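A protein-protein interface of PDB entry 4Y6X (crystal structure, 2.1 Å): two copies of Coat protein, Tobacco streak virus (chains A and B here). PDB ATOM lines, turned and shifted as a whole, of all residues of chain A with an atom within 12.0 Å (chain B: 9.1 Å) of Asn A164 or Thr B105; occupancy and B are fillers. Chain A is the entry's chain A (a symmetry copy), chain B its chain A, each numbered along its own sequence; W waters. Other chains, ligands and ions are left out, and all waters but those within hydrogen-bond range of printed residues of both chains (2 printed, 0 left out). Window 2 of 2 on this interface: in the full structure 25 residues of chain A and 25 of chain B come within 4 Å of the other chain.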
ATOM      1  N   PRO A 158      17.160  20.197  20.421  1.00  0.00           N
ATOM      2  CA  PRO A 158      17.119  21.371  21.307  1.00  0.00           C
ATOM      3  C   PRO A 158      15.748  22.005  21.258  1.00  0.00           C
ATOM      4  O   PRO A 158      15.020  21.908  20.247  1.00  0.00           O
ATOM      5  CB  PRO A 158      18.157  22.332  20.713  1.00  0.00           C
ATOM      6  CG  PRO A 158      18.861  21.622  19.601  1.00  0.00           C
ATOM      7  CD  PRO A 158      18.240  20.251  19.402  1.00  0.00           C
ATOM      8  N   GLU A 159      15.377  22.635  22.345  1.00  0.00           N
ATOM      9  CA  GLU A 159      14.077  23.265  22.506  1.00  0.00           C
ATOM     10  C   GLU A 159      13.795  24.309  21.399  1.00  0.00           C
ATOM     11  O   GLU A 159      12.669  24.453  20.950  1.00  0.00           O
ATOM     12  CB  GLU A 159      14.007  23.939  23.884  1.00  0.00           C
ATOM     13  N   ASP A 160      14.812  25.022  20.954  1.00  0.00           N
ATOM     14  CA  ASP A 160      14.617  26.011  19.913  1.00  0.00           C
ATOM     15  C   ASP A 160      14.767  25.435  18.491  1.00  0.00           C
ATOM     16  O   ASP A 160      14.880  26.193  17.523  1.00  0.00           O
ATOM     17  CB  ASP A 160      15.549  27.225  20.134  1.00  0.00           C
ATOM     18  CG  ASP A 160      17.001  26.834  20.389  1.00  0.00           C
ATOM     19  OD1 ASP A 160      17.292  25.633  20.635  1.00  0.00           O
ATOM     20  OD2 ASP A 160      17.859  27.751  20.360  1.00  0.00           O
ATOM     21  N   PHE A 161      14.693  24.113  18.325  1.00  0.00           N
ATOM     22  CA  PHE A 161      14.840  23.579  16.985  1.00  0.00           C
ATOM     23  C   PHE A 161      13.723  23.973  16.008  1.00  0.00           C
ATOM     24  O   PHE A 161      14.000  24.218  14.804  1.00  0.00           O
ATOM     25  CB  PHE A 161      15.023  22.098  16.986  1.00  0.00           C
ATOM     26  CG  PHE A 161      15.637  21.568  15.726  1.00  0.00           C
ATOM     27  CD1 PHE A 161      14.869  21.282  14.641  1.00  0.00           C
ATOM     28  CD2 PHE A 161      16.999  21.459  15.612  1.00  0.00           C
ATOM     29  CE1 PHE A 161      15.459  20.823  13.462  1.00  0.00           C
ATOM     30  CE2 PHE A 161      17.579  20.986  14.491  1.00  0.00           C
ATOM     31  CZ  PHE A 161      16.810  20.645  13.412  1.00  0.00           C
ATOM     32  N   LEU A 162      12.482  24.031  16.480  1.00  0.00           N
ATOM     33  CA  LEU A 162      11.364  24.268  15.582  1.00  0.00           C
ATOM     34  C   LEU A 162      10.835  25.701  15.624  1.00  0.00           C
ATOM     35  O   LEU A 162       9.700  25.929  15.277  1.00  0.00           O
ATOM     36  CB  LEU A 162      10.226  23.244  15.797  1.00  0.00           C
ATOM     37  CG  LEU A 162      10.539  21.817  15.404  1.00  0.00           C
ATOM     38  CD1 LEU A 162       9.427  20.876  15.862  1.00  0.00           C
ATOM     39  CD2 LEU A 162      10.789  21.668  13.895  1.00  0.00           C
ATOM     40  N   VAL A 163      11.676  26.651  16.001  1.00  0.00           N
ATOM     41  CA  VAL A 163      11.442  28.078  15.731  1.00  0.00           C
ATOM     42  C   VAL A 163      11.220  28.255  14.224  1.00  0.00           C
ATOM     43  O   VAL A 163      11.904  27.627  13.407  1.00  0.00           O
ATOM     44  CB  VAL A 163      12.649  28.923  16.175  1.00  0.00           C
ATOM     45  CG1 VAL A 163      12.621  30.320  15.540  1.00  0.00           C
ATOM     46  CG2 VAL A 163      12.704  29.012  17.713  1.00  0.00           C
ATOM     47  N   ASN A 164      10.195  29.044  13.870  1.00  0.00           N
ATOM     48  CA  ASN A 164       9.897  29.442  12.467  1.00  0.00           C
ATOM     49  C   ASN A 164       9.696  28.200  11.596  1.00  0.00           C
ATOM     50  O   ASN A 164      10.355  28.031  10.515  1.00  0.00           O
ATOM     51  CB  ASN A 164      11.018  30.356  11.904  1.00  0.00           C
ATOM     52  CG  ASN A 164      10.582  31.109  10.650  1.00  0.00           C
ATOM     53  OD1 ASN A 164       9.392  31.275  10.441  1.00  0.00           O
ATOM     54  ND2 ASN A 164      11.528  31.488   9.772  1.00  0.00           N
ATOM     55  N   GLN A 165       8.797  27.323  12.073  1.00  0.00           N
ATOM     56  CA  GLN A 165       8.437  26.075  11.366  1.00  0.00           C
ATOM     57  C   GLN A 165       7.138  26.237  10.595  1.00  0.00           C
ATOM     58  O   GLN A 165       6.815  27.337  10.212  1.00  0.00           O
ATOM     59  CB  GLN A 165       8.307  24.868  12.299  1.00  0.00           C
ATOM     60  CG  GLN A 165       6.923  24.751  12.903  1.00  0.00           C
ATOM     61  CD  GLN A 165       6.754  23.537  13.807  1.00  0.00           C
ATOM     62  OE1 GLN A 165       6.718  23.670  15.036  1.00  0.00           O
ATOM     63  NE2 GLN A 165       6.684  22.355  13.208  1.00  0.00           N
ATOM     64  N   ILE B  69      14.405  19.355  10.006  1.00  0.00           N
ATOM     65  CA  ILE B  69      15.528  20.080   9.531  1.00  0.00           C
ATOM     66  C   ILE B  69      15.449  21.541   9.914  1.00  0.00           C
ATOM     67  O   ILE B  69      14.347  22.127  10.066  1.00  0.00           O
ATOM     68  CB  ILE B  69      15.766  19.882   8.067  1.00  0.00           C
ATOM     69  CG1 ILE B  69      14.694  20.501   7.261  1.00  0.00           C
ATOM     70  CG2 ILE B  69      15.834  18.406   7.629  1.00  0.00           C
ATOM     71  CD1 ILE B  69      15.345  21.200   6.116  1.00  0.00           C
ATOM     72  N   GLY B  70      16.610  22.137  10.101  1.00  0.00           N
ATOM     73  CA  GLY B  70      16.688  23.567  10.393  1.00  0.00           C
ATOM     74  C   GLY B  70      17.833  24.130   9.633  1.00  0.00           C
ATOM     75  O   GLY B  70      18.835  23.449   9.448  1.00  0.00           O
ATOM     76  N   PHE B  71      17.708  25.355   9.192  1.00  0.00           N
ATOM     77  CA  PHE B  71      18.757  25.979   8.432  1.00  0.00           C
ATOM     78  C   PHE B  71      18.662  27.465   8.454  1.00  0.00           C
ATOM     79  O   PHE B  71      17.606  28.039   8.784  1.00  0.00           O
ATOM     80  CB  PHE B  71      18.782  25.469   7.004  1.00  0.00           C
ATOM     81  CG  PHE B  71      17.570  25.848   6.214  1.00  0.00           C
ATOM     82  CD1 PHE B  71      16.449  25.027   6.220  1.00  0.00           C
ATOM     83  CD2 PHE B  71      17.561  26.995   5.442  1.00  0.00           C
ATOM     84  CE1 PHE B  71      15.303  25.355   5.500  1.00  0.00           C
ATOM     85  CE2 PHE B  71      16.413  27.350   4.717  1.00  0.00           C
ATOM     86  CZ  PHE B  71      15.289  26.523   4.766  1.00  0.00           C
ATOM     87  N   VAL B  72      19.776  28.090   8.117  1.00  0.00           N
ATOM     88  CA  VAL B  72      19.843  29.512   7.801  1.00  0.00           C
ATOM     89  C   VAL B  72      20.428  29.652   6.407  1.00  0.00           C
ATOM     90  O   VAL B  72      21.406  28.976   6.073  1.00  0.00           O
ATOM     91  CB  VAL B  72      20.754  30.269   8.800  1.00  0.00           C
ATOM     92  CG1 VAL B  72      20.853  31.734   8.434  1.00  0.00           C
ATOM     93  CG2 VAL B  72      20.123  30.260  10.166  1.00  0.00           C
ATOM     94  N   ALA B  73      19.855  30.510   5.565  1.00  0.00           N
ATOM     95  CA  ALA B  73      20.393  30.718   4.200  1.00  0.00           C
ATOM     96  C   ALA B  73      20.897  32.171   4.002  1.00  0.00           C
ATOM     97  O   ALA B  73      20.451  33.104   4.664  1.00  0.00           O
ATOM     98  CB  ALA B  73      19.307  30.439   3.190  1.00  0.00           C
ATOM     99  N   VAL B  74      21.771  32.376   3.042  1.00  0.00           N
ATOM    100  CA  VAL B  74      22.243  33.729   2.717  1.00  0.00           C
ATOM    101  C   VAL B  74      21.336  34.494   1.710  1.00  0.00           C
ATOM    102  O   VAL B  74      21.654  35.601   1.332  1.00  0.00           O
ATOM    103  CB  VAL B  74      23.684  33.720   2.152  1.00  0.00           C
ATOM    104  CG1 VAL B  74      24.634  33.120   3.160  1.00  0.00           C
ATOM    105  CG2 VAL B  74      23.761  32.951   0.837  1.00  0.00           C
ATOM    106  N   SER B  75      20.212  33.911   1.302  1.00  0.00           N
ATOM    107  CA  SER B  75      19.294  34.577   0.375  1.00  0.00           C
ATOM    108  C   SER B  75      17.863  34.088   0.692  1.00  0.00           C
ATOM    109  O   SER B  75      17.687  33.078   1.356  1.00  0.00           O
ATOM    110  CB  SER B  75      19.689  34.163  -1.052  1.00  0.00           C
ATOM    111  OG  SER B  75      18.583  34.216  -1.921  1.00  0.00           O
ATOM    112  N   ASP B  76      16.857  34.821   0.217  1.00  0.00           N
ATOM    113  CA  ASP B  76      15.479  34.325   0.185  1.00  0.00           C
ATOM    114  C   ASP B  76      15.430  33.128  -0.744  1.00  0.00           C
ATOM    115  O   ASP B  76      16.263  32.968  -1.609  1.00  0.00           O
ATOM    116  CB  ASP B  76      14.505  35.380  -0.327  1.00  0.00           C
ATOM    117  CG  ASP B  76      14.338  36.585   0.615  1.00  0.00           C
ATOM    118  OD1 ASP B  76      15.168  36.844   1.526  1.00  0.00           O
ATOM    119  OD2 ASP B  76      13.330  37.315   0.427  1.00  0.00           O
ATOM    120  N   PHE B  79      12.056  25.897  -0.459  1.00  0.00           N
ATOM    121  CA  PHE B  79      12.508  24.563  -0.295  1.00  0.00           C
ATOM    122  C   PHE B  79      11.400  23.577  -0.077  1.00  0.00           C
ATOM    123  O   PHE B  79      10.305  23.914   0.358  1.00  0.00           O
ATOM    124  CB  PHE B  79      13.508  24.497   0.854  1.00  0.00           C
ATOM    125  CG  PHE B  79      12.875  24.459   2.204  1.00  0.00           C
ATOM    126  CD1 PHE B  79      12.190  25.580   2.733  1.00  0.00           C
ATOM    127  CD2 PHE B  79      12.989  23.320   2.966  1.00  0.00           C
ATOM    128  CE1 PHE B  79      11.631  25.551   4.020  1.00  0.00           C
ATOM    129  CE2 PHE B  79      12.423  23.272   4.226  1.00  0.00           C
ATOM    130  CZ  PHE B  79      11.727  24.370   4.758  1.00  0.00           C
ATOM    131  N   LEU B  99       7.897  25.496   0.563  1.00  0.00           N
ATOM    132  CA  LEU B  99       7.790  26.610   1.503  1.00  0.00           C
ATOM    133  C   LEU B  99       8.884  27.640   1.248  1.00  0.00           C
ATOM    134  O   LEU B  99       9.937  27.308   0.800  1.00  0.00           O
ATOM    135  CB  LEU B  99       7.984  26.087   2.914  1.00  0.00           C
ATOM    136  CG  LEU B  99       6.829  25.294   3.519  1.00  0.00           C
ATOM    137  CD1 LEU B  99       7.258  24.853   4.929  1.00  0.00           C
ATOM    138  CD2 LEU B  99       5.546  26.142   3.568  1.00  0.00           C
ATOM    139  N   GLY B 100       8.625  28.883   1.606  1.00  0.00           N
ATOM    140  CA  GLY B 100       9.559  29.976   1.498  1.00  0.00           C
ATOM    141  C   GLY B 100      10.422  30.130   2.747  1.00  0.00           C
ATOM    142  O   GLY B 100      10.090  29.599   3.831  1.00  0.00           O
ATOM    143  N   PHE B 101      11.562  30.793   2.565  1.00  0.00           N
ATOM    144  CA  PHE B 101      12.427  31.254   3.654  1.00  0.00           C
ATOM    145  C   PHE B 101      13.042  32.582   3.297  1.00  0.00           C
ATOM    146  O   PHE B 101      13.062  32.952   2.144  1.00  0.00           O
ATOM    147  CB  PHE B 101      13.542  30.234   3.961  1.00  0.00           C
ATOM    148  CG  PHE B 101      14.398  29.862   2.801  1.00  0.00           C
ATOM    149  CD1 PHE B 101      15.488  30.616   2.447  1.00  0.00           C
ATOM    150  CD2 PHE B 101      14.152  28.717   2.099  1.00  0.00           C
ATOM    151  CE1 PHE B 101      16.295  30.243   1.386  1.00  0.00           C
ATOM    152  CE2 PHE B 101      14.934  28.319   1.069  1.00  0.00           C
ATOM    153  CZ  PHE B 101      16.002  29.090   0.704  1.00  0.00           C
ATOM    154  N   LYS B 102      13.541  33.277   4.310  1.00  0.00           N
ATOM    155  CA  LYS B 102      14.147  34.593   4.196  1.00  0.00           C
ATOM    156  C   LYS B 102      15.627  34.582   4.541  1.00  0.00           C
ATOM    157  O   LYS B 102      16.087  33.740   5.295  1.00  0.00           O
ATOM    158  CB  LYS B 102      13.455  35.549   5.165  1.00  0.00           C
ATOM    159  CG  LYS B 102      11.947  35.729   4.898  1.00  0.00           C
ATOM    160  CD  LYS B 102      11.693  36.180   3.454  1.00  0.00           C
ATOM    161  N   LYS B 103      16.354  35.549   3.999  1.00  0.00           N
ATOM    162  CA  LYS B 103      17.773  35.661   4.192  1.00  0.00           C
ATOM    163  C   LYS B 103      18.065  35.789   5.657  1.00  0.00           C
ATOM    164  O   LYS B 103      17.368  36.479   6.361  1.00  0.00           O
ATOM    165  CB  LYS B 103      18.261  36.892   3.455  1.00  0.00           C
ATOM    166  CG  LYS B 103      19.708  37.229   3.682  1.00  0.00           C
ATOM    167  CD  LYS B 103      20.169  38.427   2.873  1.00  0.00           C
ATOM    168  CE  LYS B 103      19.623  39.743   3.455  1.00  0.00           C
ATOM    169  NZ  LYS B 103      20.761  40.445   4.114  1.00  0.00           N
ATOM    170  N   ASN B 104      19.127  35.132   6.115  1.00  0.00           N
ATOM    171  CA  ASN B 104      19.600  35.215   7.494  1.00  0.00           C
ATOM    172  C   ASN B 104      18.536  35.009   8.533  1.00  0.00           C
ATOM    173  O   ASN B 104      18.606  35.575   9.579  1.00  0.00           O
ATOM    174  CB  ASN B 104      20.227  36.583   7.745  1.00  0.00           C
ATOM    175  CG  ASN B 104      21.485  36.813   6.926  1.00  0.00           C
ATOM    176  OD1 ASN B 104      22.165  35.868   6.503  1.00  0.00           O
ATOM    177  ND2 ASN B 104      21.798  38.069   6.693  1.00  0.00           N
ATOM    178  N   THR B 105      17.553  34.200   8.261  1.00  0.00           N
ATOM    179  CA  THR B 105      16.514  33.903   9.236  1.00  0.00           C
ATOM    180  C   THR B 105      16.375  32.392   9.390  1.00  0.00           C
ATOM    181  O   THR B 105      16.118  31.653   8.437  1.00  0.00           O
ATOM    182  CB  THR B 105      15.197  34.538   8.759  1.00  0.00           C
ATOM    183  OG1 THR B 105      15.436  35.952   8.581  1.00  0.00           O
ATOM    184  CG2 THR B 105      14.111  34.395   9.763  1.00  0.00           C
ATOM    185  N   TYR B 106      16.585  31.914  10.605  1.00  0.00           N
ATOM    186  CA  TYR B 106      16.426  30.474  10.888  1.00  0.00           C
ATOM    187  C   TYR B 106      15.052  30.022  10.401  1.00  0.00           C
ATOM    188  O   TYR B 106      14.034  30.622  10.707  1.00  0.00           O
ATOM    189  CB  TYR B 106      16.593  30.196  12.376  1.00  0.00           C
ATOM    190  CG  TYR B 106      16.465  28.726  12.703  1.00  0.00           C
ATOM    191  CD1 TYR B 106      17.557  27.842  12.540  1.00  0.00           C
ATOM    192  CD2 TYR B 106      15.257  28.189  13.176  1.00  0.00           C
ATOM    193  CE1 TYR B 106      17.462  26.485  12.809  1.00  0.00           C
ATOM    194  CE2 TYR B 106      15.155  26.838  13.493  1.00  0.00           C
ATOM    195  CZ  TYR B 106      16.264  25.987  13.338  1.00  0.00           C
ATOM    196  OH  TYR B 106      16.185  24.660  13.662  1.00  0.00           O
ATOM    197  N   ARG B 107      15.017  28.925   9.701  1.00  0.00           N
ATOM    198  CA  ARG B 107      13.795  28.287   9.263  1.00  0.00           C
ATOM    199  C   ARG B 107      13.840  26.827   9.625  1.00  0.00           C
ATOM    200  O   ARG B 107      14.880  26.165   9.501  1.00  0.00           O
ATOM    201  CB  ARG B 107      13.749  28.452   7.768  1.00  0.00           C
ATOM    202  CG  ARG B 107      12.584  27.877   7.061  1.00  0.00           C
ATOM    203  CD  ARG B 107      11.393  28.576   7.635  1.00  0.00           C
ATOM    204  NE  ARG B 107      10.400  28.883   6.636  1.00  0.00           N
ATOM    205  CZ  ARG B 107       9.092  28.854   6.847  1.00  0.00           C
ATOM    206  NH1 ARG B 107       8.577  28.597   8.055  1.00  0.00           N
ATOM    207  NH2 ARG B 107       8.284  29.095   5.824  1.00  0.00           N
ATOM    208  N   SER B 108      12.731  26.268  10.047  1.00  0.00           N
ATOM    209  CA  SER B 108      12.740  24.842  10.281  1.00  0.00           C
ATOM    210  C   SER B 108      11.524  24.174   9.698  1.00  0.00           C
ATOM    211  O   SER B 108      10.622  24.837   9.244  1.00  0.00           O
ATOM    212  CB  SER B 108      12.837  24.581  11.767  1.00  0.00           C
ATOM    213  OG  SER B 108      11.728  25.112  12.433  1.00  0.00           O
ATOM    214  N   ARG B 109      11.552  22.852   9.623  1.00  0.00           N
ATOM    215  CA  ARG B 109      10.450  22.082   9.061  1.00  0.00           C
ATOM    216  C   ARG B 109      10.455  20.685   9.610  1.00  0.00           C
ATOM    217  O   ARG B 109      11.540  20.089   9.763  1.00  0.00           O
ATOM    218  CB  ARG B 109      10.587  22.012   7.530  1.00  0.00           C
ATOM    219  CG  ARG B 109       9.509  21.277   6.746  1.00  0.00           C
ATOM    220  CD  ARG B 109       8.323  22.059   6.342  1.00  0.00           C
ATOM    221  NE  ARG B 109       7.779  21.585   5.070  1.00  0.00           N
ATOM    222  CZ  ARG B 109       6.955  20.537   4.905  1.00  0.00           C
ATOM    223  NH1 ARG B 109       6.534  19.799   5.929  1.00  0.00           N
ATOM    224  NH2 ARG B 109       6.527  20.228   3.678  1.00  0.00           N
ATOM    225  N   ASP B 110       9.267  20.195   9.944  1.00  0.00           N
ATOM    226  CA  ASP B 110       9.034  18.791  10.328  1.00  0.00           C
ATOM    227  C   ASP B 110       8.390  18.054   9.197  1.00  0.00           C
ATOM    228  O   ASP B 110       7.329  18.443   8.750  1.00  0.00           O
ATOM    229  CB  ASP B 110       8.060  18.798  11.499  1.00  0.00           C
ATOM    230  N   GLN B 141      23.216  26.809   5.584  1.00  0.00           N
ATOM    231  CA  GLN B 141      23.892  26.165   6.703  1.00  0.00           C
ATOM    232  C   GLN B 141      22.845  25.389   7.484  1.00  0.00           C
ATOM    233  O   GLN B 141      21.897  25.988   8.001  1.00  0.00           O
ATOM    234  CB  GLN B 141      24.592  27.193   7.604  1.00  0.00           C
ATOM    235  CG  GLN B 141      25.550  28.077   6.827  1.00  0.00           C
ATOM    236  CD  GLN B 141      25.959  29.271   7.646  1.00  0.00           C
ATOM    237  OE1 GLN B 141      26.326  29.134   8.806  1.00  0.00           O
ATOM    238  NE2 GLN B 141      25.852  30.416   7.079  1.00  0.00           N
HETATM  239  O   HOH W   1       6.035  27.450   7.503  1.00  0.00           O
HETATM  240  O   HOH W   2       7.093  22.211  10.144  1.00  0.00           O
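OH of Tyr B106 sits at hydrogen-bond distance from O of Phe A161, 2.5 Å away. The side-chain amide nitrogen of Asn A164 lies within hydrogen-bond range of the backbone carbonyl oxygen of Tyr B106 (2.8 Å). The guanidinium group of Arg B107 sits at hydrogen-bond distance from the backbone carbonyl oxygen of Asn A164, 3.1 Å away. NH1 of Arg B107 is in hydrogen-bond range of O of Gln A165, at 3.1 Å. The backbone carbonyl oxygen (O) of Phe A161 lies close to the side-chain hydroxyl (OG) of Ser B108. The side-chain hydroxyl (OG) of Ser B108 sits at hydrogen-bond distance from the backbone carbonyl oxygen (O) of Val A163. The backbone NH of Ser B108 lies within hydrogen-bond range of the backbone carbonyl oxygen of Asn A164 (3.0 Å).
The backbone carbonyl oxygen of Ile B69 lies within hydrogen-bond range of the backbone NH of Arg B109, at 2.9 Å. O of Phe B71 sits at hydrogen-bond distance from N of Arg B107 (2.9 Å). The backbone carbonyl oxygen (O) of Gly B100 sits at hydrogen-bond distance from the guanidinium group (NH2) of Arg B107. OG1 of Thr B105 sits at hydrogen-bond distance from O of Lys B103 (3.0 Å).
Phe A161 touches Ile B69. Phe A161 touches Gly B70 (CZ to N, 3.6 Å). CA of Leu A162 touches OG of Ser B108 (3.3 Å). CE2 of Tyr B106 touches O of Val A163 (3.3 Å). Asn A164 touches Thr B105 (ND2 to CG2, 3.9 Å). Gln A165 touches Ser B108.
Of the printed residues of chain B, Phe A161 touches Ile B69 (3.6 Å), Gly B70 (3.6 Å), Tyr B106 (2.5 Å) and Ser B108 (3.3 Å). Of the printed residues of chain B, Leu A162 touches Ser B108. Of chain B, only Tyr B106 (3.3 Å) and Ser B108 (2.7 Å) come within 4 Å of Val A163. Of chain B, only Thr B105, Tyr B106, Arg B107 and Ser B108 come within 4 Å of Asn A164. Of the printed residues of chain B, Gln A165 touches Arg B107 and Ser B108. Printed residues of chain A within 4 Å of Ile B69: Phe A161. Of the printed residues of chain A, Gly B70 touches Phe A161. No residue of chain A comes within 4 Å of Phe B71. No residue of chain A comes within 4 Å of Ala B73. No residue of chain A comes within 4 Å of Lys B102. No residue of chain A comes within 4 Å of Asn B104. Thr B105 touches just one residue of chain A: Asn A164. Arg B107 touches just these residues of chain A: Asn A164 (3.1 Å) and Gln A165 (3.1 Å). Arg B109 touches none of the printed residues of chain A. The nearest residue of chain B that does not touch Asn A164 is Arg B109 (5.4 Å). The nearest printed residue of chain B that does not touch Gln A165 is Asp B110 (4.2 Å).
Hydrophobic or aromatic side chains of chain B within 4 Å of the printed part of chain A: Tyr B106. Of the 8 printed residues of chain A, 5 touch a printed residue of chain B. Among the printed residues, 13 pairs touch across the chains.
No position is printed for both chains.
Water W1 bridges the backbone carbonyl oxygen of Gln A165 (2.8 Å) and the guanidinium group of Arg B107 (2.8 Å). Water W2 lies within hydrogen-bond range of the backbone NH of Asp B110 and the side-chain amide nitrogen of Gln A165.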
